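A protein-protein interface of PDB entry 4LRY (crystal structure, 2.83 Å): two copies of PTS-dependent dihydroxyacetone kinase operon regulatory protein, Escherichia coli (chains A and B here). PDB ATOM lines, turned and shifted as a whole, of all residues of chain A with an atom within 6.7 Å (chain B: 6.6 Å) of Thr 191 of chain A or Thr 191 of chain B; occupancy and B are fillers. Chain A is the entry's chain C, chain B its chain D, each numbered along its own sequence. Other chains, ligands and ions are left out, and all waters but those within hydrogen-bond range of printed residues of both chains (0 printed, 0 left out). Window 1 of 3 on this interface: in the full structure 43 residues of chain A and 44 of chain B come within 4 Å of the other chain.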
ATOM      1  N   GLY A 186       2.077 -17.541  15.080  1.00  0.00           N
ATOM      2  CA  GLY A 186       2.021 -16.675  16.261  1.00  0.00           C
ATOM      3  C   GLY A 186       3.320 -15.956  16.672  1.00  0.00           C
ATOM      4  O   GLY A 186       3.335 -14.720  16.740  1.00  0.00           O
ATOM      5  N   ASN A 187       4.387 -16.710  16.974  1.00  0.00           N
ATOM      6  CA  ASN A 187       5.705 -16.119  17.304  1.00  0.00           C
ATOM      7  C   ASN A 187       6.388 -15.298  16.218  1.00  0.00           C
ATOM      8  O   ASN A 187       7.053 -14.324  16.528  1.00  0.00           O
ATOM      9  CB  ASN A 187       6.698 -17.154  17.780  1.00  0.00           C
ATOM     10  CG  ASN A 187       6.363 -17.685  19.137  1.00  0.00           C
ATOM     11  OD1 ASN A 187       6.271 -16.949  20.110  1.00  0.00           O
ATOM     12  ND2 ASN A 187       6.212 -18.966  19.226  1.00  0.00           N
ATOM     13  N   LEU A 188       6.251 -15.669  14.958  1.00  0.00           N
ATOM     14  CA  LEU A 188       6.726 -14.782  13.933  1.00  0.00           C
ATOM     15  C   LEU A 188       5.958 -13.465  13.957  1.00  0.00           C
ATOM     16  O   LEU A 188       6.582 -12.416  13.966  1.00  0.00           O
ATOM     17  CB  LEU A 188       6.739 -15.455  12.573  1.00  0.00           C
ATOM     18  CG  LEU A 188       8.052 -16.068  12.019  1.00  0.00           C
ATOM     19  CD1 LEU A 188       9.253 -16.141  12.962  1.00  0.00           C
ATOM     20  CD2 LEU A 188       7.770 -17.425  11.381  1.00  0.00           C
ATOM     21  N   LEU A 189       4.624 -13.470  14.034  1.00  0.00           N
ATOM     22  CA  LEU A 189       3.907 -12.162  14.188  1.00  0.00           C
ATOM     23  C   LEU A 189       4.546 -11.268  15.247  1.00  0.00           C
ATOM     24  O   LEU A 189       4.974 -10.150  14.947  1.00  0.00           O
ATOM     25  CB  LEU A 189       2.449 -12.330  14.531  1.00  0.00           C
ATOM     26  CG  LEU A 189       1.527 -12.818  13.427  1.00  0.00           C
ATOM     27  CD1 LEU A 189       0.055 -12.721  13.910  1.00  0.00           C
ATOM     28  CD2 LEU A 189       1.726 -12.064  12.096  1.00  0.00           C
ATOM     29  N   LEU A 190       4.623 -11.772  16.479  1.00  0.00           N
ATOM     30  CA  LEU A 190       5.113 -10.966  17.580  1.00  0.00           C
ATOM     31  C   LEU A 190       6.517 -10.448  17.280  1.00  0.00           C
ATOM     32  O   LEU A 190       6.793  -9.243  17.404  1.00  0.00           O
ATOM     33  CB  LEU A 190       5.037 -11.718  18.916  1.00  0.00           C
ATOM     34  CG  LEU A 190       6.085 -11.416  20.018  1.00  0.00           C
ATOM     35  CD1 LEU A 190       6.201  -9.914  20.493  1.00  0.00           C
ATOM     36  CD2 LEU A 190       5.850 -12.328  21.232  1.00  0.00           C
ATOM     37  N   THR A 191       7.406 -11.336  16.850  1.00  0.00           N
ATOM     38  CA  THR A 191       8.778 -10.896  16.685  1.00  0.00           C
ATOM     39  C   THR A 191       9.016 -10.187  15.346  1.00  0.00           C
ATOM     40  O   THR A 191       9.755  -9.262  15.312  1.00  0.00           O
ATOM     41  CB  THR A 191       9.867 -11.951  17.118  1.00  0.00           C
ATOM     42  OG1 THR A 191      10.712 -12.281  16.018  1.00  0.00           O
ATOM     43  CG2 THR A 191       9.293 -13.186  17.765  1.00  0.00           C
ATOM     44  N   ASP A 192       8.341 -10.562  14.271  1.00  0.00           N
ATOM     45  CA  ASP A 192       8.317  -9.754  13.043  1.00  0.00           C
ATOM     46  C   ASP A 192       7.921  -8.272  13.288  1.00  0.00           C
ATOM     47  O   ASP A 192       8.531  -7.345  12.744  1.00  0.00           O
ATOM     48  CB  ASP A 192       7.332 -10.365  12.037  1.00  0.00           C
ATOM     49  CG  ASP A 192       8.017 -11.230  10.982  1.00  0.00           C
ATOM     50  OD1 ASP A 192       9.223 -11.531  11.112  1.00  0.00           O
ATOM     51  OD2 ASP A 192       7.341 -11.624  10.012  1.00  0.00           O
ATOM     52  N   SER A 193       6.893  -8.046  14.096  1.00  0.00           N
ATOM     53  CA  SER A 193       6.478  -6.711  14.378  1.00  0.00           C
ATOM     54  C   SER A 193       7.449  -6.011  15.351  1.00  0.00           C
ATOM     55  O   SER A 193       7.641  -4.784  15.253  1.00  0.00           O
ATOM     56  CB  SER A 193       5.076  -6.723  14.915  1.00  0.00           C
ATOM     57  OG  SER A 193       5.161  -7.064  16.262  1.00  0.00           O
ATOM     58  N   LEU A 194       8.094  -6.741  16.268  1.00  0.00           N
ATOM     59  CA  LEU A 194       9.174  -6.087  17.024  1.00  0.00           C
ATOM     60  C   LEU A 194      10.256  -5.609  16.084  1.00  0.00           C
ATOM     61  O   LEU A 194      10.739  -4.508  16.268  1.00  0.00           O
ATOM     62  CB  LEU A 194       9.784  -6.937  18.139  1.00  0.00           C
ATOM     63  CG  LEU A 194       9.083  -7.107  19.504  1.00  0.00           C
ATOM     64  CD1 LEU A 194      10.113  -7.216  20.643  1.00  0.00           C
ATOM     65  CD2 LEU A 194       8.062  -6.005  19.811  1.00  0.00           C
ATOM     66  N   LEU A 195      10.617  -6.419  15.084  1.00  0.00           N
ATOM     67  CA  LEU A 195      11.542  -6.019  14.010  1.00  0.00           C
ATOM     68  C   LEU A 195      11.035  -4.756  13.303  1.00  0.00           C
ATOM     69  O   LEU A 195      11.708  -3.736  13.348  1.00  0.00           O
ATOM     70  CB  LEU A 195      11.689  -7.129  12.963  1.00  0.00           C
ATOM     71  CG  LEU A 195      13.014  -7.580  12.327  1.00  0.00           C
ATOM     72  CD1 LEU A 195      12.845  -7.689  10.811  1.00  0.00           C
ATOM     73  CD2 LEU A 195      14.190  -6.704  12.694  1.00  0.00           C
ATOM     74  N   ALA A 196       9.839  -4.826  12.693  1.00  0.00           N
ATOM     75  CA  ALA A 196       9.172  -3.670  12.068  1.00  0.00           C
ATOM     76  C   ALA A 196       9.399  -2.361  12.833  1.00  0.00           C
ATOM     77  O   ALA A 196       9.928  -1.394  12.269  1.00  0.00           O
ATOM     78  CB  ALA A 196       7.706  -3.935  11.909  1.00  0.00           C
ATOM     79  N   GLY B 186      13.779 -22.276  13.577  1.00  0.00           N
ATOM     80  CA  GLY B 186      14.727 -21.841  12.606  1.00  0.00           C
ATOM     81  C   GLY B 186      14.452 -20.440  12.201  1.00  0.00           C
ATOM     82  O   GLY B 186      15.359 -19.613  12.216  1.00  0.00           O
ATOM     83  N   ASN B 187      13.205 -20.172  11.816  1.00  0.00           N
ATOM     84  CA  ASN B 187      12.746 -18.819  11.484  1.00  0.00           C
ATOM     85  C   ASN B 187      12.818 -17.815  12.620  1.00  0.00           C
ATOM     86  O   ASN B 187      13.224 -16.693  12.417  1.00  0.00           O
ATOM     87  CB  ASN B 187      11.342 -18.900  10.982  1.00  0.00           C
ATOM     88  CG  ASN B 187      11.309 -19.238   9.565  1.00  0.00           C
ATOM     89  OD1 ASN B 187      12.209 -18.854   8.859  1.00  0.00           O
ATOM     90  ND2 ASN B 187      10.291 -19.941   9.112  1.00  0.00           N
ATOM     91  N   LEU B 188      12.428 -18.218  13.816  1.00  0.00           N
ATOM     92  CA  LEU B 188      12.650 -17.410  14.968  1.00  0.00           C
ATOM     93  C   LEU B 188      14.118 -17.100  15.248  1.00  0.00           C
ATOM     94  O   LEU B 188      14.399 -15.993  15.680  1.00  0.00           O
ATOM     95  CB  LEU B 188      11.999 -18.025  16.187  1.00  0.00           C
ATOM     96  CG  LEU B 188      10.795 -17.361  16.878  1.00  0.00           C
ATOM     97  CD1 LEU B 188      10.143 -16.352  15.994  1.00  0.00           C
ATOM     98  CD2 LEU B 188       9.777 -18.397  17.394  1.00  0.00           C
ATOM     99  N   LEU B 189      15.080 -18.010  15.022  1.00  0.00           N
ATOM    100  CA  LEU B 189      16.525 -17.599  15.199  1.00  0.00           C
ATOM    101  C   LEU B 189      17.014 -16.597  14.126  1.00  0.00           C
ATOM    102  O   LEU B 189      17.756 -15.650  14.427  1.00  0.00           O
ATOM    103  CB  LEU B 189      17.492 -18.774  15.230  1.00  0.00           C
ATOM    104  CG  LEU B 189      17.490 -19.918  16.233  1.00  0.00           C
ATOM    105  CD1 LEU B 189      18.162 -21.074  15.502  1.00  0.00           C
ATOM    106  CD2 LEU B 189      18.156 -19.700  17.616  1.00  0.00           C
ATOM    107  N   LEU B 190      16.601 -16.819  12.883  1.00  0.00           N
ATOM    108  CA  LEU B 190      16.909 -15.885  11.809  1.00  0.00           C
ATOM    109  C   LEU B 190      16.484 -14.473  12.104  1.00  0.00           C
ATOM    110  O   LEU B 190      17.260 -13.516  11.956  1.00  0.00           O
ATOM    111  CB  LEU B 190      16.241 -16.315  10.508  1.00  0.00           C
ATOM    112  CG  LEU B 190      17.336 -16.624   9.478  1.00  0.00           C
ATOM    113  CD1 LEU B 190      17.204 -18.127   8.830  1.00  0.00           C
ATOM    114  CD2 LEU B 190      17.569 -15.404   8.461  1.00  0.00           C
ATOM    115  N   THR B 191      15.220 -14.335  12.497  1.00  0.00           N
ATOM    116  CA  THR B 191      14.687 -13.018  12.619  1.00  0.00           C
ATOM    117  C   THR B 191      15.091 -12.534  13.998  1.00  0.00           C
ATOM    118  O   THR B 191      15.322 -11.358  14.176  1.00  0.00           O
ATOM    119  CB  THR B 191      13.193 -12.886  12.223  1.00  0.00           C
ATOM    120  OG1 THR B 191      12.411 -12.640  13.375  1.00  0.00           O
ATOM    121  CG2 THR B 191      12.687 -14.095  11.453  1.00  0.00           C
ATOM    122  N   ASP B 192      15.300 -13.448  14.937  1.00  0.00           N
ATOM    123  CA  ASP B 192      15.939 -13.054  16.184  1.00  0.00           C
ATOM    124  C   ASP B 192      17.285 -12.357  16.001  1.00  0.00           C
ATOM    125  O   ASP B 192      17.633 -11.442  16.757  1.00  0.00           O
ATOM    126  CB  ASP B 192      16.139 -14.247  17.079  1.00  0.00           C
ATOM    127  CG  ASP B 192      15.079 -14.357  18.150  1.00  0.00           C
ATOM    128  OD1 ASP B 192      13.962 -13.774  18.018  1.00  0.00           O
ATOM    129  OD2 ASP B 192      15.376 -15.069  19.133  1.00  0.00           O
ATOM    130  N   SER B 193      18.062 -12.774  15.011  1.00  0.00           N
ATOM    131  CA  SER B 193      19.370 -12.180  14.889  1.00  0.00           C
ATOM    132  C   SER B 193      19.387 -11.028  13.921  1.00  0.00           C
ATOM    133  O   SER B 193      20.310 -10.216  14.013  1.00  0.00           O
ATOM    134  CB  SER B 193      20.454 -13.211  14.560  1.00  0.00           C
ATOM    135  OG  SER B 193      20.546 -13.434  13.166  1.00  0.00           O
ATOM    136  N   LEU B 194      18.420 -10.961  12.998  1.00  0.00           N
ATOM    137  CA  LEU B 194      18.201  -9.719  12.230  1.00  0.00           C
ATOM    138  C   LEU B 194      17.873  -8.610  13.194  1.00  0.00           C
ATOM    139  O   LEU B 194      18.482  -7.560  13.139  1.00  0.00           O
ATOM    140  CB  LEU B 194      17.028  -9.808  11.291  1.00  0.00           C
ATOM    141  CG  LEU B 194      17.260 -10.181   9.848  1.00  0.00           C
ATOM    142  CD1 LEU B 194      16.490 -11.494   9.607  1.00  0.00           C
ATOM    143  CD2 LEU B 194      16.818  -9.045   8.933  1.00  0.00           C
ATOM    144  N   LEU B 195      16.904  -8.851  14.066  1.00  0.00           N
ATOM    145  CA  LEU B 195      16.614  -7.987  15.189  1.00  0.00           C
ATOM    146  C   LEU B 195      17.837  -7.612  16.057  1.00  0.00           C
ATOM    147  O   LEU B 195      17.915  -6.483  16.519  1.00  0.00           O
ATOM    148  CB  LEU B 195      15.526  -8.606  16.077  1.00  0.00           C
ATOM    149  CG  LEU B 195      14.447  -7.743  16.734  1.00  0.00           C
ATOM    150  CD1 LEU B 195      13.866  -8.503  17.878  1.00  0.00           C
ATOM    151  CD2 LEU B 195      14.932  -6.421  17.275  1.00  0.00           C
ATOM    152  N   ALA B 196      18.778  -8.518  16.327  1.00  0.00           N
ATOM    153  CA  ALA B 196      19.971  -8.073  17.090  1.00  0.00           C
ATOM    154  C   ALA B 196      20.772  -7.086  16.256  1.00  0.00           C
ATOM    155  O   ALA B 196      21.019  -5.949  16.688  1.00  0.00           O
ATOM    156  CB  ALA B 196      20.831  -9.226  17.537  1.00  0.00           C
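Printed residues of chain B within 4 Å of Leu 188 of chain A: Asn 187 (3.9 Å) and Leu 188 (3.2 Å). Thr 191 of chain A touches just these residues of chain B: Leu 188 and Thr 191. Printed residues of chain B within 4 Å of Leu 195 of chain A: Leu 195 (3.7 Å). Leu 189 of chain B touches none of the printed residues of chain A. Thr 191 of chain B touches one residue of chain A. Leu 194 of chain B touches none of the printed residues of chain A.
Hydrophobic or aromatic side chains of chain B that line the printed part of chain A: Leu 188. Hydrophobic or aromatic side chains of chain A within 4 Å of the printed part of chain B: Leu 188 and Leu 195. Along chain A the printed residues that touch a printed residue of chain B span positions 187 to 195. Among the printed residues, 6 pairs touch across the chains. Among the printed residues, no Asp or Glu carboxylate lies within 4 Å of a Lys or Arg side-chain nitrogen of the other chain.
Leu 188 of chain B touches its own counterpart, Leu 188 of chain A. Thr 191 of chain A touches Leu 188 of chain B, but with the chains exchanged Leu 188 of chain A does not touch Thr 191 of chain B (4.3 Å). Thr 191 of chain A touches its own counterpart, Thr 191 of chain B. Leu 195 of chain A touches its own counterpart, Leu 195 of chain B.
The side-chain hydroxyl (OG1) of Thr 191 of chain A is in hydrogen-bond range of the side-chain hydroxyl (OG1) of Thr 191 of chain B (3.2 Å).
Among the printed residues, pairs that only touch across the chains: Leu 188 of chain A with Leu 188 of chain B (3.2 Å), Asn 187 of chain A with Leu 188 of chain B (3.3 Å), Leu 195 of chain A with Leu 195 of chain B (3.7 Å), Thr 191 of chain A with Leu 188 of chain B (3.7 Å) and Leu 188 of chain A with Asn 187 of chain B (3.9 Å).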
